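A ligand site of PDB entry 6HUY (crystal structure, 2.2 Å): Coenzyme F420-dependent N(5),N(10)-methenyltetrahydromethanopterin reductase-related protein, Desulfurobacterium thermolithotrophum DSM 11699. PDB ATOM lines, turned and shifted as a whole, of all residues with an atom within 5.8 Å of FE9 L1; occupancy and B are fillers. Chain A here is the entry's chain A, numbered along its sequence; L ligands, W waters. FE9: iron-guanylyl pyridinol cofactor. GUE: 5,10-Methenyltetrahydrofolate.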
ATOM      1  N   VAL A   5       3.002  -7.451   0.244  1.00  0.00           N
ATOM      2  CA  VAL A   5       2.849  -6.986   1.615  1.00  0.00           C
ATOM      3  C   VAL A   5       2.932  -8.215   2.513  1.00  0.00           C
ATOM      4  O   VAL A   5       2.135  -9.154   2.376  1.00  0.00           O
ATOM      5  CB  VAL A   5       1.512  -6.256   1.810  1.00  0.00           C
ATOM      6  CG1 VAL A   5       1.361  -5.852   3.254  1.00  0.00           C
ATOM      7  CG2 VAL A   5       1.448  -5.034   0.927  1.00  0.00           C
ATOM      8  N   TYR A   6       3.897  -8.221   3.425  1.00  0.00           N
ATOM      9  CA  TYR A   6       4.076  -9.324   4.364  1.00  0.00           C
ATOM     10  C   TYR A   6       3.361  -8.939   5.646  1.00  0.00           C
ATOM     11  O   TYR A   6       3.770  -8.018   6.353  1.00  0.00           O
ATOM     12  CB  TYR A   6       5.554  -9.609   4.605  1.00  0.00           C
ATOM     13  CG  TYR A   6       6.218 -10.272   3.422  1.00  0.00           C
ATOM     14  CD1 TYR A   6       6.158 -11.650   3.260  1.00  0.00           C
ATOM     15  CD2 TYR A   6       6.873  -9.518   2.460  1.00  0.00           C
ATOM     16  CE1 TYR A   6       6.738 -12.265   2.169  1.00  0.00           C
ATOM     17  CE2 TYR A   6       7.453 -10.119   1.368  1.00  0.00           C
ATOM     18  CZ  TYR A   6       7.386 -11.488   1.234  1.00  0.00           C
ATOM     19  OH  TYR A   6       7.956 -12.102   0.147  1.00  0.00           O
ATOM     20  N   GLY A   7       2.278  -9.649   5.954  1.00  0.00           N
ATOM     21  CA  GLY A   7       1.512  -9.408   7.153  1.00  0.00           C
ATOM     22  C   GLY A   7       0.131  -8.850   6.878  1.00  0.00           C
ATOM     23  O   GLY A   7      -0.008  -7.779   6.271  1.00  0.00           O
ATOM     24  N   PHE A   8      -0.896  -9.570   7.333  1.00  0.00           N
ATOM     25  CA  PHE A   8      -2.269  -9.122   7.168  1.00  0.00           C
ATOM     26  C   PHE A   8      -2.643  -8.076   8.204  1.00  0.00           C
ATOM     27  O   PHE A   8      -3.401  -7.146   7.915  1.00  0.00           O
ATOM     28  CB  PHE A   8      -3.214 -10.325   7.268  1.00  0.00           C
ATOM     29  CG  PHE A   8      -4.630 -10.033   6.866  1.00  0.00           C
ATOM     30  CD1 PHE A   8      -5.533  -9.502   7.763  1.00  0.00           C
ATOM     31  CD2 PHE A   8      -5.060 -10.324   5.578  1.00  0.00           C
ATOM     32  CE1 PHE A   8      -6.847  -9.254   7.387  1.00  0.00           C
ATOM     33  CE2 PHE A   8      -6.377 -10.069   5.195  1.00  0.00           C
ATOM     34  CZ  PHE A   8      -7.264  -9.538   6.100  1.00  0.00           C
ATOM     35  N   GLY A   9      -2.135  -8.222   9.420  1.00  0.00           N
ATOM     36  CA  GLY A   9      -2.531  -7.370  10.536  1.00  0.00           C
ATOM     37  C   GLY A   9      -3.385  -8.176  11.493  1.00  0.00           C
ATOM     38  O   GLY A   9      -4.244  -8.982  11.081  1.00  0.00           O
ATOM     39  N   SER A  10      -3.150  -7.972  12.783  1.00  0.00           N
ATOM     40  CA  SER A  10      -3.883  -8.715  13.811  1.00  0.00           C
ATOM     41  C   SER A  10      -5.335  -8.249  13.857  1.00  0.00           C
ATOM     42  O   SER A  10      -5.626  -7.168  14.365  1.00  0.00           O
ATOM     43  CB  SER A  10      -3.205  -8.548  15.169  1.00  0.00           C
ATOM     44  OG  SER A  10      -4.012  -9.112  16.192  1.00  0.00           O
ATOM     45  N   TYR A  13      -6.200  -7.696  17.686  1.00  0.00           N
ATOM     46  CA  TYR A  13      -5.743  -6.514  18.418  1.00  0.00           C
ATOM     47  C   TYR A  13      -6.556  -5.280  18.064  1.00  0.00           C
ATOM     48  O   TYR A  13      -6.878  -4.475  18.941  1.00  0.00           O
ATOM     49  CB  TYR A  13      -4.256  -6.237  18.160  1.00  0.00           C
ATOM     50  CG  TYR A  13      -3.812  -4.984  18.881  1.00  0.00           C
ATOM     51  CD1 TYR A  13      -3.363  -5.040  20.190  1.00  0.00           C
ATOM     52  CD2 TYR A  13      -3.919  -3.736  18.276  1.00  0.00           C
ATOM     53  CE1 TYR A  13      -2.995  -3.906  20.866  1.00  0.00           C
ATOM     54  CE2 TYR A  13      -3.550  -2.589  18.951  1.00  0.00           C
ATOM     55  CZ  TYR A  13      -3.088  -2.681  20.247  1.00  0.00           C
ATOM     56  OH  TYR A  13      -2.737  -1.547  20.932  1.00  0.00           O
ATOM     57  N   TYR A  14      -6.873  -5.086  16.777  1.00  0.00           N
ATOM     58  CA  TYR A  14      -7.524  -3.853  16.344  1.00  0.00           C
ATOM     59  C   TYR A  14      -9.004  -3.792  16.711  1.00  0.00           C
ATOM     60  O   TYR A  14      -9.652  -2.781  16.410  1.00  0.00           O
ATOM     61  CB  TYR A  14      -7.345  -3.679  14.839  1.00  0.00           C
ATOM     62  CG  TYR A  14      -5.891  -3.535  14.426  1.00  0.00           C
ATOM     63  CD1 TYR A  14      -5.073  -2.566  15.001  1.00  0.00           C
ATOM     64  CD2 TYR A  14      -5.341  -4.370  13.468  1.00  0.00           C
ATOM     65  CE1 TYR A  14      -3.729  -2.432  14.614  1.00  0.00           C
ATOM     66  CE2 TYR A  14      -4.007  -4.250  13.087  1.00  0.00           C
ATOM     67  CZ  TYR A  14      -3.219  -3.287  13.670  1.00  0.00           C
ATOM     68  OH  TYR A  14      -1.908  -3.195  13.269  1.00  0.00           O
ATOM     69  N   GLY A  31      -4.477  -2.522   8.918  1.00  0.00           N
ATOM     70  CA  GLY A  31      -3.087  -2.915   8.856  1.00  0.00           C
ATOM     71  C   GLY A  31      -2.599  -3.220   7.462  1.00  0.00           C
ATOM     72  O   GLY A  31      -2.942  -2.510   6.506  1.00  0.00           O
ATOM     73  N   SER A  49       1.214 -11.974   1.834  1.00  0.00           N
ATOM     74  CA  SER A  49       1.635 -13.253   2.391  1.00  0.00           C
ATOM     75  C   SER A  49       1.480 -13.221   3.902  1.00  0.00           C
ATOM     76  O   SER A  49       1.957 -12.297   4.564  1.00  0.00           O
ATOM     77  CB  SER A  49       3.080 -13.567   2.001  1.00  0.00           C
ATOM     78  OG  SER A  49       3.371 -14.941   2.196  1.00  0.00           O
ATOM     79  N   ASP A  50       0.826 -14.253   4.444  1.00  0.00           N
ATOM     80  CA  ASP A  50       0.587 -14.364   5.875  1.00  0.00           C
ATOM     81  C   ASP A  50       0.351 -15.824   6.219  1.00  0.00           C
ATOM     82  O   ASP A  50      -0.382 -16.504   5.480  1.00  0.00           O
ATOM     83  CB  ASP A  50      -0.618 -13.502   6.285  1.00  0.00           C
ATOM     84  CG  ASP A  50      -0.772 -13.394   7.770  1.00  0.00           C
ATOM     85  OD1 ASP A  50      -1.330 -14.348   8.379  1.00  0.00           O
ATOM     86  OD2 ASP A  50      -0.348 -12.372   8.346  1.00  0.00           O
ATOM     87  N   PRO A  51       0.929 -16.352   7.301  1.00  0.00           N
ATOM     88  CA  PRO A  51       0.740 -17.773   7.603  1.00  0.00           C
ATOM     89  C   PRO A  51      -0.644 -18.106   8.120  1.00  0.00           C
ATOM     90  O   PRO A  51      -1.006 -19.292   8.140  1.00  0.00           O
ATOM     91  CB  PRO A  51       1.796 -18.065   8.688  1.00  0.00           C
ATOM     92  CG  PRO A  51       2.570 -16.798   8.879  1.00  0.00           C
ATOM     93  CD  PRO A  51       1.737 -15.684   8.329  1.00  0.00           C
ATOM     94  N   ASN A  52      -1.430 -17.113   8.559  1.00  0.00           N
ATOM     95  CA  ASN A  52      -2.739 -17.333   9.145  1.00  0.00           C
ATOM     96  C   ASN A  52      -3.864 -16.790   8.268  1.00  0.00           C
ATOM     97  O   ASN A  52      -4.873 -16.285   8.757  1.00  0.00           O
ATOM     98  CB  ASN A  52      -2.819 -16.706  10.531  1.00  0.00           C
ATOM     99  CG  ASN A  52      -1.751 -17.231  11.470  1.00  0.00           C
ATOM    100  OD1 ASN A  52      -1.909 -18.280  12.092  1.00  0.00           O
ATOM    101  ND2 ASN A  52      -0.646 -16.492  11.583  1.00  0.00           N
ATOM    102  N   ASP A  75       5.858 -17.310   1.959  1.00  0.00           N
ATOM    103  CA  ASP A  75       6.625 -16.058   1.905  1.00  0.00           C
ATOM    104  C   ASP A  75       7.630 -16.084   0.773  1.00  0.00           C
ATOM    105  O   ASP A  75       7.894 -15.038   0.158  1.00  0.00           O
ATOM    106  CB  ASP A  75       7.337 -15.802   3.235  1.00  0.00           C
ATOM    107  CG  ASP A  75       6.393 -15.459   4.367  1.00  0.00           C
ATOM    108  OD1 ASP A  75       5.261 -15.029   4.082  1.00  0.00           O
ATOM    109  OD2 ASP A  75       6.787 -15.596   5.540  1.00  0.00           O
ATOM    110  N   LEU A  87       7.130  -5.068   5.079  1.00  0.00           N
ATOM    111  CA  LEU A  87       7.108  -5.974   6.219  1.00  0.00           C
ATOM    112  C   LEU A  87       6.147  -5.408   7.259  1.00  0.00           C
ATOM    113  O   LEU A  87       6.534  -4.656   8.150  1.00  0.00           O
ATOM    114  CB  LEU A  87       8.512  -6.154   6.778  1.00  0.00           C
ATOM    115  CG  LEU A  87       9.546  -6.720   5.811  1.00  0.00           C
ATOM    116  CD1 LEU A  87      10.947  -6.608   6.405  1.00  0.00           C
ATOM    117  CD2 LEU A  87       9.200  -8.146   5.459  1.00  0.00           C
ATOM    118  N   PHE A  88       4.877  -5.803   7.146  1.00  0.00           N
ATOM    119  CA  PHE A  88       3.884  -5.533   8.194  1.00  0.00           C
ATOM    120  C   PHE A  88       3.898  -6.685   9.191  1.00  0.00           C
ATOM    121  O   PHE A  88       2.906  -7.372   9.434  1.00  0.00           O
ATOM    122  CB  PHE A  88       2.496  -5.341   7.578  1.00  0.00           C
ATOM    123  CG  PHE A  88       1.584  -4.486   8.409  1.00  0.00           C
ATOM    124  CD1 PHE A  88       0.797  -5.052   9.405  1.00  0.00           C
ATOM    125  CD2 PHE A  88       1.538  -3.119   8.226  1.00  0.00           C
ATOM    126  CE1 PHE A  88      -0.029  -4.258  10.191  1.00  0.00           C
ATOM    127  CE2 PHE A  88       0.718  -2.318   9.001  1.00  0.00           C
ATOM    128  CZ  PHE A  88      -0.055  -2.891   9.982  1.00  0.00           C
ATOM    129  N   THR A  89       5.078  -6.901   9.760  1.00  0.00           N
ATOM    130  CA  THR A  89       5.418  -8.086  10.519  1.00  0.00           C
ATOM    131  C   THR A  89       5.463  -7.812  12.021  1.00  0.00           C
ATOM    132  O   THR A  89       5.529  -6.659  12.449  1.00  0.00           O
ATOM    133  CB  THR A  89       6.776  -8.622  10.027  1.00  0.00           C
ATOM    134  OG1 THR A  89       7.703  -7.538   9.947  1.00  0.00           O
ATOM    135  CG2 THR A  89       6.628  -9.248   8.660  1.00  0.00           C
ATOM    136  N   PRO A  90       5.469  -8.858  12.844  1.00  0.00           N
ATOM    137  CA  PRO A  90       5.212  -8.671  14.278  1.00  0.00           C
ATOM    138  C   PRO A  90       6.313  -7.909  15.018  1.00  0.00           C
ATOM    139  O   PRO A  90       7.457  -7.800  14.579  1.00  0.00           O
ATOM    140  CB  PRO A  90       5.098 -10.107  14.804  1.00  0.00           C
ATOM    141  CG  PRO A  90       4.758 -10.920  13.625  1.00  0.00           C
ATOM    142  CD  PRO A  90       5.482 -10.287  12.484  1.00  0.00           C
ATOM    143  N   PHE A  91       5.925  -7.409  16.202  1.00  0.00           N
ATOM    144  CA  PHE A  91       6.816  -6.657  17.080  1.00  0.00           C
ATOM    145  C   PHE A  91       7.886  -7.540  17.714  1.00  0.00           C
ATOM    146  O   PHE A  91       9.047  -7.136  17.812  1.00  0.00           O
ATOM    147  CB  PHE A  91       5.991  -6.000  18.197  1.00  0.00           C
ATOM    148  CG  PHE A  91       5.467  -4.632  17.862  1.00  0.00           C
ATOM    149  CD1 PHE A  91       6.330  -3.572  17.665  1.00  0.00           C
ATOM    150  CD2 PHE A  91       4.094  -4.399  17.822  1.00  0.00           C
ATOM    151  CE1 PHE A  91       5.850  -2.310  17.380  1.00  0.00           C
ATOM    152  CE2 PHE A  91       3.599  -3.136  17.530  1.00  0.00           C
ATOM    153  CZ  PHE A  91       4.479  -2.091  17.324  1.00  0.00           C
ATOM    154  N   VAL A  95      10.617 -12.206  14.291  1.00  0.00           N
ATOM    155  CA  VAL A  95       9.947 -12.741  13.106  1.00  0.00           C
ATOM    156  C   VAL A  95      10.286 -11.910  11.886  1.00  0.00           C
ATOM    157  O   VAL A  95      10.353 -12.427  10.763  1.00  0.00           O
ATOM    158  CB  VAL A  95       8.425 -12.819  13.346  1.00  0.00           C
ATOM    159  CG1 VAL A  95       7.733 -13.495  12.175  1.00  0.00           C
ATOM    160  CG2 VAL A  95       8.111 -13.548  14.646  1.00  0.00           C
ATOM    161  N   ILE A  99      11.769 -13.307   8.458  1.00  0.00           N
ATOM    162  CA  ILE A  99      11.142 -13.162   7.146  1.00  0.00           C
ATOM    163  C   ILE A  99      12.092 -12.458   6.188  1.00  0.00           C
ATOM    164  O   ILE A  99      12.266 -12.887   5.044  1.00  0.00           O
ATOM    165  CB  ILE A  99       9.795 -12.414   7.258  1.00  0.00           C
ATOM    166  CG1 ILE A  99       8.783 -13.228   8.067  1.00  0.00           C
ATOM    167  CG2 ILE A  99       9.213 -12.131   5.870  1.00  0.00           C
ATOM    168  CD1 ILE A  99       7.692 -12.370   8.649  1.00  0.00           C
ATOM    169  N   THR A 116       7.881  -1.314   8.596  1.00  0.00           N
ATOM    170  CA  THR A 116       6.846  -0.445   9.132  1.00  0.00           C
ATOM    171  C   THR A 116       7.226  -0.091  10.574  1.00  0.00           C
ATOM    172  O   THR A 116       8.417  -0.110  10.914  1.00  0.00           O
ATOM    173  CB  THR A 116       5.469  -1.120   9.035  1.00  0.00           C
ATOM    174  OG1 THR A 116       5.510  -2.400   9.668  1.00  0.00           O
ATOM    175  CG2 THR A 116       5.049  -1.311   7.587  1.00  0.00           C
ATOM    176  N   CYS A 117       6.249   0.229  11.435  1.00  0.00           N
ATOM    177  CA  CYS A 117       6.565   0.652  12.797  1.00  0.00           C
ATOM    178  C   CYS A 117       7.196  -0.445  13.647  1.00  0.00           C
ATOM    179  O   CYS A 117       7.754  -0.151  14.705  1.00  0.00           O
ATOM    180  CB  CYS A 117       5.295   1.137  13.499  1.00  0.00           C
ATOM    181  SG  CYS A 117       4.372  -0.198  14.265  1.00  0.00           S
ATOM    182  N   THR A 118       7.089  -1.709  13.259  1.00  0.00           N
ATOM    183  CA  THR A 118       7.589  -2.774  14.115  1.00  0.00           C
ATOM    184  C   THR A 118       9.086  -2.995  13.983  1.00  0.00           C
ATOM    185  O   THR A 118       9.627  -3.833  14.707  1.00  0.00           O
ATOM    186  CB  THR A 118       6.836  -4.074  13.817  1.00  0.00           C
ATOM    187  OG1 THR A 118       6.991  -4.426  12.442  1.00  0.00           O
ATOM    188  CG2 THR A 118       5.326  -3.929  14.166  1.00  0.00           C
ATOM    189  N   HIS A 146       6.255   3.382   6.338  1.00  0.00           N
ATOM    190  CA  HIS A 146       5.732   3.523   7.682  1.00  0.00           C
ATOM    191  C   HIS A 146       4.441   4.357   7.657  1.00  0.00           C
ATOM    192  O   HIS A 146       4.506   5.539   7.315  1.00  0.00           O
ATOM    193  CB  HIS A 146       6.784   4.200   8.571  1.00  0.00           C
ATOM    194  CG  HIS A 146       6.514   4.098  10.027  1.00  0.00           C
ATOM    195  ND1 HIS A 146       5.257   4.265  10.569  1.00  0.00           N
ATOM    196  CD2 HIS A 146       7.337   3.853  11.076  1.00  0.00           C
ATOM    197  CE1 HIS A 146       5.316   4.120  11.880  1.00  0.00           C
ATOM    198  NE2 HIS A 146       6.574   3.880  12.214  1.00  0.00           N
ATOM    199  N   PRO A 147       3.281   3.784   7.979  1.00  0.00           N
ATOM    200  CA  PRO A 147       2.029   4.549   7.863  1.00  0.00           C
ATOM    201  C   PRO A 147       1.835   5.599   8.938  1.00  0.00           C
ATOM    202  O   PRO A 147       0.952   6.452   8.783  1.00  0.00           O
ATOM    203  CB  PRO A 147       0.949   3.457   7.977  1.00  0.00           C
ATOM    204  CG  PRO A 147       1.585   2.409   8.831  1.00  0.00           C
ATOM    205  CD  PRO A 147       3.045   2.405   8.442  1.00  0.00           C
ATOM    206  N   ALA A 148       2.594   5.548  10.042  1.00  0.00           N
ATOM    207  CA  ALA A 148       2.480   6.525  11.124  1.00  0.00           C
ATOM    208  C   ALA A 148       1.015   6.754  11.463  1.00  0.00           C
ATOM    209  O   ALA A 148       0.552   7.884  11.646  1.00  0.00           O
ATOM    210  CB  ALA A 148       3.167   7.846  10.766  1.00  0.00           C
ATOM    211  N   ALA A 149       0.278   5.642  11.498  1.00  0.00           N
ATOM    212  CA  ALA A 149      -1.172   5.573  11.635  1.00  0.00           C
ATOM    213  C   ALA A 149      -1.559   4.130  11.377  1.00  0.00           C
ATOM    214  O   ALA A 149      -0.737   3.346  10.882  1.00  0.00           O
ATOM    215  CB  ALA A 149      -1.879   6.497  10.637  1.00  0.00           C
ATOM    216  N   ILE A 150      -2.786   3.756  11.683  1.00  0.00           N
ATOM    217  CA  ILE A 150      -3.279   2.401  11.431  1.00  0.00           C
ATOM    218  C   ILE A 150      -3.912   2.395  10.037  1.00  0.00           C
ATOM    219  O   ILE A 150      -4.947   3.060   9.848  1.00  0.00           O
ATOM    220  CB  ILE A 150      -4.275   1.965  12.513  1.00  0.00           C
ATOM    221  CG1 ILE A 150      -3.574   1.911  13.872  1.00  0.00           C
ATOM    222  CG2 ILE A 150      -4.861   0.608  12.151  1.00  0.00           C
ATOM    223  CD1 ILE A 150      -4.480   1.569  15.071  1.00  0.00           C
ATOM    224  N   PRO A 151      -3.313   1.727   9.050  1.00  0.00           N
ATOM    225  CA  PRO A 151      -3.935   1.688   7.722  1.00  0.00           C
ATOM    226  C   PRO A 151      -5.357   1.154   7.783  1.00  0.00           C
ATOM    227  O   PRO A 151      -5.625   0.115   8.391  1.00  0.00           O
ATOM    228  CB  PRO A 151      -3.011   0.763   6.919  1.00  0.00           C
ATOM    229  CG  PRO A 151      -1.702   0.846   7.619  1.00  0.00           C
ATOM    230  CD  PRO A 151      -2.015   1.042   9.075  1.00  0.00           C
ATOM    231  N   GLY A 203       7.418   8.384  13.466  1.00  0.00           N
ATOM    232  CA  GLY A 203       6.276   7.586  13.077  1.00  0.00           C
ATOM    233  C   GLY A 203       5.727   6.663  14.146  1.00  0.00           C
ATOM    234  O   GLY A 203       4.510   6.436  14.203  1.00  0.00           O
ATOM    235  N   ASP A 204       6.598   6.119  14.992  1.00  0.00           N
ATOM    236  CA  ASP A 204       6.150   5.156  16.000  1.00  0.00           C
ATOM    237  C   ASP A 204       5.239   5.826  17.019  1.00  0.00           C
ATOM    238  O   ASP A 204       4.982   7.035  16.985  1.00  0.00           O
ATOM    239  CB  ASP A 204       7.347   4.505  16.681  1.00  0.00           C
ATOM    240  CG  ASP A 204       8.168   3.627  15.747  1.00  0.00           C
ATOM    241  OD1 ASP A 204       7.897   3.597  14.521  1.00  0.00           O
ATOM    242  OD2 ASP A 204       9.084   2.942  16.266  1.00  0.00           O
HETATM  243  O2  FE9 L   1       0.285  -1.584  15.573  1.00  0.00           O
HETATM  244 FE   FE9 L   1       1.758   0.080  13.365  1.00  0.00          FE
HETATM  245  C1F FE9 L   1       0.210   0.122  12.421  1.00  0.00           C
HETATM  246  O1F FE9 L   1      -0.756   0.064  11.873  1.00  0.00           O
HETATM  247  C2F FE9 L   1       1.966   1.836  12.966  1.00  0.00           C
HETATM  248  O2F FE9 L   1       1.999   2.944  12.698  1.00  0.00           O
HETATM  249  C8  FE9 L   1       2.729  -0.448  11.853  1.00  0.00           C
HETATM  250  O18 FE9 L   1       3.173   0.353  11.044  1.00  0.00           O
HETATM  251  C7  FE9 L   1       2.963  -1.920  11.633  1.00  0.00           C
HETATM  252  C6  FE9 L   1       2.233  -2.616  12.770  1.00  0.00           C
HETATM  253  N1  FE9 L   1       1.518  -1.827  13.697  1.00  0.00           N
HETATM  254  C5  FE9 L   1       2.212  -4.098  12.879  1.00  0.00           C
HETATM  255  C5M FE9 L   1       2.924  -4.954  11.866  1.00  0.00           C
HETATM  256  C4  FE9 L   1       1.469  -4.709  14.005  1.00  0.00           C
HETATM  257  C3  FE9 L   1       0.786  -3.827  14.985  1.00  0.00           C
HETATM  258  C3M FE9 L   1       0.038  -4.459  16.123  1.00  0.00           C
HETATM  259  C2  FE9 L   1       0.739  -2.370  14.729  1.00  0.00           C
HETATM  260  O3P FE9 L   1       1.436  -6.062  14.165  1.00  0.00           O
HETATM  261  P1  FE9 L   1       0.204  -6.988  13.683  1.00  0.00           P
HETATM  262  O1P FE9 L   1      -1.015  -6.161  13.540  1.00  0.00           O
HETATM  263  O2P FE9 L   1       0.030  -8.154  14.774  1.00  0.00           O
HETATM  264  O5' FE9 L   1       0.662  -7.604  12.280  1.00  0.00           O
HETATM  265  C5' FE9 L   1       1.697  -8.575  12.220  1.00  0.00           C
HETATM  266  C4' FE9 L   1       1.306  -9.546  11.127  1.00  0.00           C
HETATM  267  O4' FE9 L   1       2.423 -10.341  10.739  1.00  0.00           O
HETATM  268  C1' FE9 L   1       1.930 -11.641  10.439  1.00  0.00           C
HETATM  269  C2' FE9 L   1       0.818 -11.885  11.458  1.00  0.00           C
HETATM  270  O2' FE9 L   1      -0.119 -12.848  10.978  1.00  0.00           O
HETATM  271  C3' FE9 L   1       0.202 -10.498  11.588  1.00  0.00           C
HETATM  272  O3' FE9 L   1      -0.934 -10.365  10.725  1.00  0.00           O
HETATM  273  N9A FE9 L   1       2.971 -12.701  10.482  1.00  0.00           N
HETATM  274  C4A FE9 L   1       3.650 -13.119   9.413  1.00  0.00           C
HETATM  275  N3A FE9 L   1       3.660 -12.778   8.108  1.00  0.00           N
HETATM  276  C2A FE9 L   1       4.483 -13.391   7.239  1.00  0.00           C
HETATM  277  N2A FE9 L   1       4.453 -13.006   5.938  1.00  0.00           N
HETATM  278  N1A FE9 L   1       5.338 -14.377   7.605  1.00  0.00           N
HETATM  279  C6A FE9 L   1       5.425 -14.829   8.868  1.00  0.00           C
HETATM  280  O6A FE9 L   1       6.237 -15.730   9.191  1.00  0.00           O
HETATM  281  C5A FE9 L   1       4.547 -14.173   9.886  1.00  0.00           C
HETATM  282  N7A FE9 L   1       4.326 -14.310  11.203  1.00  0.00           N
HETATM  283  C8A FE9 L   1       3.364 -13.408  11.555  1.00  0.00           C
HETATM  284  N1  GUE L   2       0.185   6.207  15.813  1.00  0.00           N
HETATM  285  C2  GUE L   2       1.422   6.353  15.291  1.00  0.00           C
HETATM  286  N3  GUE L   2       2.308   5.346  15.295  1.00  0.00           N
HETATM  287  C4  GUE L   2       2.046   4.140  15.800  1.00  0.00           C
HETATM  288  C6  GUE L   2      -1.187   2.400  16.762  1.00  0.00           C
HETATM  289  C1' GUE L   2       1.307  -2.384  20.139  1.00  0.00           C
HETATM  290  C2' GUE L   2       2.091  -1.229  20.190  1.00  0.00           C
HETATM  291  C3' GUE L   2       1.673  -0.081  19.521  1.00  0.00           C
HETATM  292  C4' GUE L   2       0.480  -0.096  18.821  1.00  0.00           C
HETATM  293  C5' GUE L   2      -0.287  -1.253  18.761  1.00  0.00           C
HETATM  294  O4  GUE L   2       2.897   3.231  15.773  1.00  0.00           O
HETATM  295  C4A GUE L   2       0.704   3.907  16.388  1.00  0.00           C
HETATM  296  N5  GUE L   2       0.216   2.730  16.957  1.00  0.00           N
HETATM  297  C7  GUE L   2      -1.928   3.589  17.373  1.00  0.00           C
HETATM  298  N8  GUE L   2      -1.470   4.881  16.866  1.00  0.00           N
HETATM  299  C8A GUE L   2      -0.229   5.034  16.350  1.00  0.00           C
HETATM  300  N2  GUE L   2       1.761   7.556  14.760  1.00  0.00           N
HETATM  301  C9  GUE L   2      -1.336   1.177  17.672  1.00  0.00           C
HETATM  302  N10 GUE L   2       0.047   1.029  18.105  1.00  0.00           N
HETATM  303  C6' GUE L   2       0.119  -2.407  19.428  1.00  0.00           C
HETATM  304  C11 GUE L   2       1.766  -3.630  20.851  1.00  0.00           C
HETATM  305  O11 GUE L   2       2.605  -3.550  21.732  1.00  0.00           O
HETATM  306  N   GUE L   2       1.281  -4.814  20.472  1.00  0.00           N
HETATM  307  CA  GUE L   2       1.948  -6.010  20.951  1.00  0.00           C
HETATM  308  C   GUE L   2       2.308  -6.925  19.816  1.00  0.00           C
HETATM  309  OX1 GUE L   2       3.208  -7.784  20.003  1.00  0.00           O
HETATM  310  OX2 GUE L   2       1.711  -6.772  18.728  1.00  0.00           O
HETATM  311  CB  GUE L   2       1.095  -6.742  21.987  1.00  0.00           C
HETATM  312  CG  GUE L   2      -0.345  -6.891  21.494  1.00  0.00           C
HETATM  313  CD  GUE L   2      -1.265  -7.422  22.578  1.00  0.00           C
HETATM  314  OE1 GUE L   2      -1.648  -8.611  22.497  1.00  0.00           O
HETATM  315  OE2 GUE L   2      -1.628  -6.642  23.509  1.00  0.00           O
HETATM  316  C1  GUE L   2       0.839   1.942  17.724  1.00  0.00           C
HETATM  317  O   HOH W   1       2.828  -7.590  16.157  1.00  0.00           O
HETATM  318  O   HOH W   2      -3.330 -11.784  11.207  1.00  0.00           O
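OD1 of Asp 75 lies within hydrogen-bond range of OG of Ser 49 (2.7 Å). The backbone carbonyl oxygen (O) of Asp 75 is in hydrogen-bond range of the side-chain hydroxyl (OH) of Tyr 6. N of Tyr 13 is in hydrogen-bond range of OG of Ser 10, at 3.0 Å. The backbone carbonyl oxygen of Ser 49 lies within hydrogen-bond range of the backbone NH of Gly 7 (3.0 Å). N of Ser 49 sits at hydrogen-bond distance from O of Val 5. The backbone carbonyl oxygen of Pro 151 is in hydrogen-bond range of the backbone NH of Gly 31 (2.9 Å). OG1 of Thr 116 sits at hydrogen-bond distance from O of Leu 87, at 2.9 Å. NE2 of His 146 sits at hydrogen-bond distance from OD1 of Asp 204, at 2.7 Å.
Water W2 bridges an oxygen (O3') of FE9 L1 (2.8 Å) and the backbone carbonyl oxygen (O) of Gly 9 (2.9 Å). Water W1 lies within hydrogen-bond range of O3P of FE9 L1 (2.9 Å), OX2 of GUE L2 (2.9 Å) and N of Phe 91 (3.1 Å).
An oxygen (O2') of FE9 L1 lies within hydrogen-bond range of the side-chain carboxylate (OD2) of Asp 50 (2.7 Å). N of Cys 117 is in hydrogen-bond range of O18 of FE9 L1 (3.1 Å). An iron atom (FE) of FE9 L1 is bound by the side-chain sulfur (SG) of Cys 117. The backbone NH (N) of Gly 9 sits at hydrogen-bond distance from an oxygen (O3') of FE9 L1, at 2.8 Å. N1A of FE9 L1 sits at hydrogen-bond distance from OD2 of Asp 75 (2.8 Å). The backbone NH (N) of Ser 10 sits at hydrogen-bond distance from an oxygen (O1P) of FE9 L1. A nitrogen (N2A) of FE9 L1 is in hydrogen-bond range of the backbone carbonyl oxygen of Ser 49. The side-chain hydroxyl of Tyr 14 is in hydrogen-bond range of an oxygen (O1P) of FE9 L1. O2F of FE9 L1 lies within hydrogen-bond range of N of Ala 149 (3.4 Å). An oxygen (O3') of FE9 L1 is in hydrogen-bond range of the backbone NH (N) of Phe 8, 3.5 Å away. The backbone carbonyl oxygen of Ala 148 sits at hydrogen-bond distance from a nitrogen (N2) of GUE L2 (3.4 Å). A nitrogen (N2) of GUE L2 lies within hydrogen-bond range of the backbone carbonyl oxygen (O) of Gly 203, at 3.0 Å.
The backbone carbonyl oxygen (O) of Phe 88 lies close to an oxygen (O4') of FE9 L1, at 3.3 Å. Merely in contact with FE9 L1: Thr 89 (3.2 Å), Pro 151 (3.2 Å), Thr 116 (3.3 Å), Ile 99 (3.3 Å), Pro 147 (3.3 Å), Thr 118 (3.4 Å), Pro 51 (3.4 Å), Tyr 6 (3.5 Å), Ile 150 (3.5 Å), Pro 90 (3.5 Å), His 146 (3.6 Å), Val 95 (3.6 Å), Asn 52 (3.7 Å), Ala 148 (3.8 Å), Gly 7 (3.8 Å) and Phe 91 (3.9 Å). Hydrophobic or aromatic side chains that line FE9 L1: Tyr 6, Tyr 14, Pro 51, Phe 88, Pro 90, Phe 91, Val 95, Ile 99, His 146, Pro 147, Ile 150 and Pro 151. Of the 32 residues printed, 26 come within 4 Å of FE9 L1.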
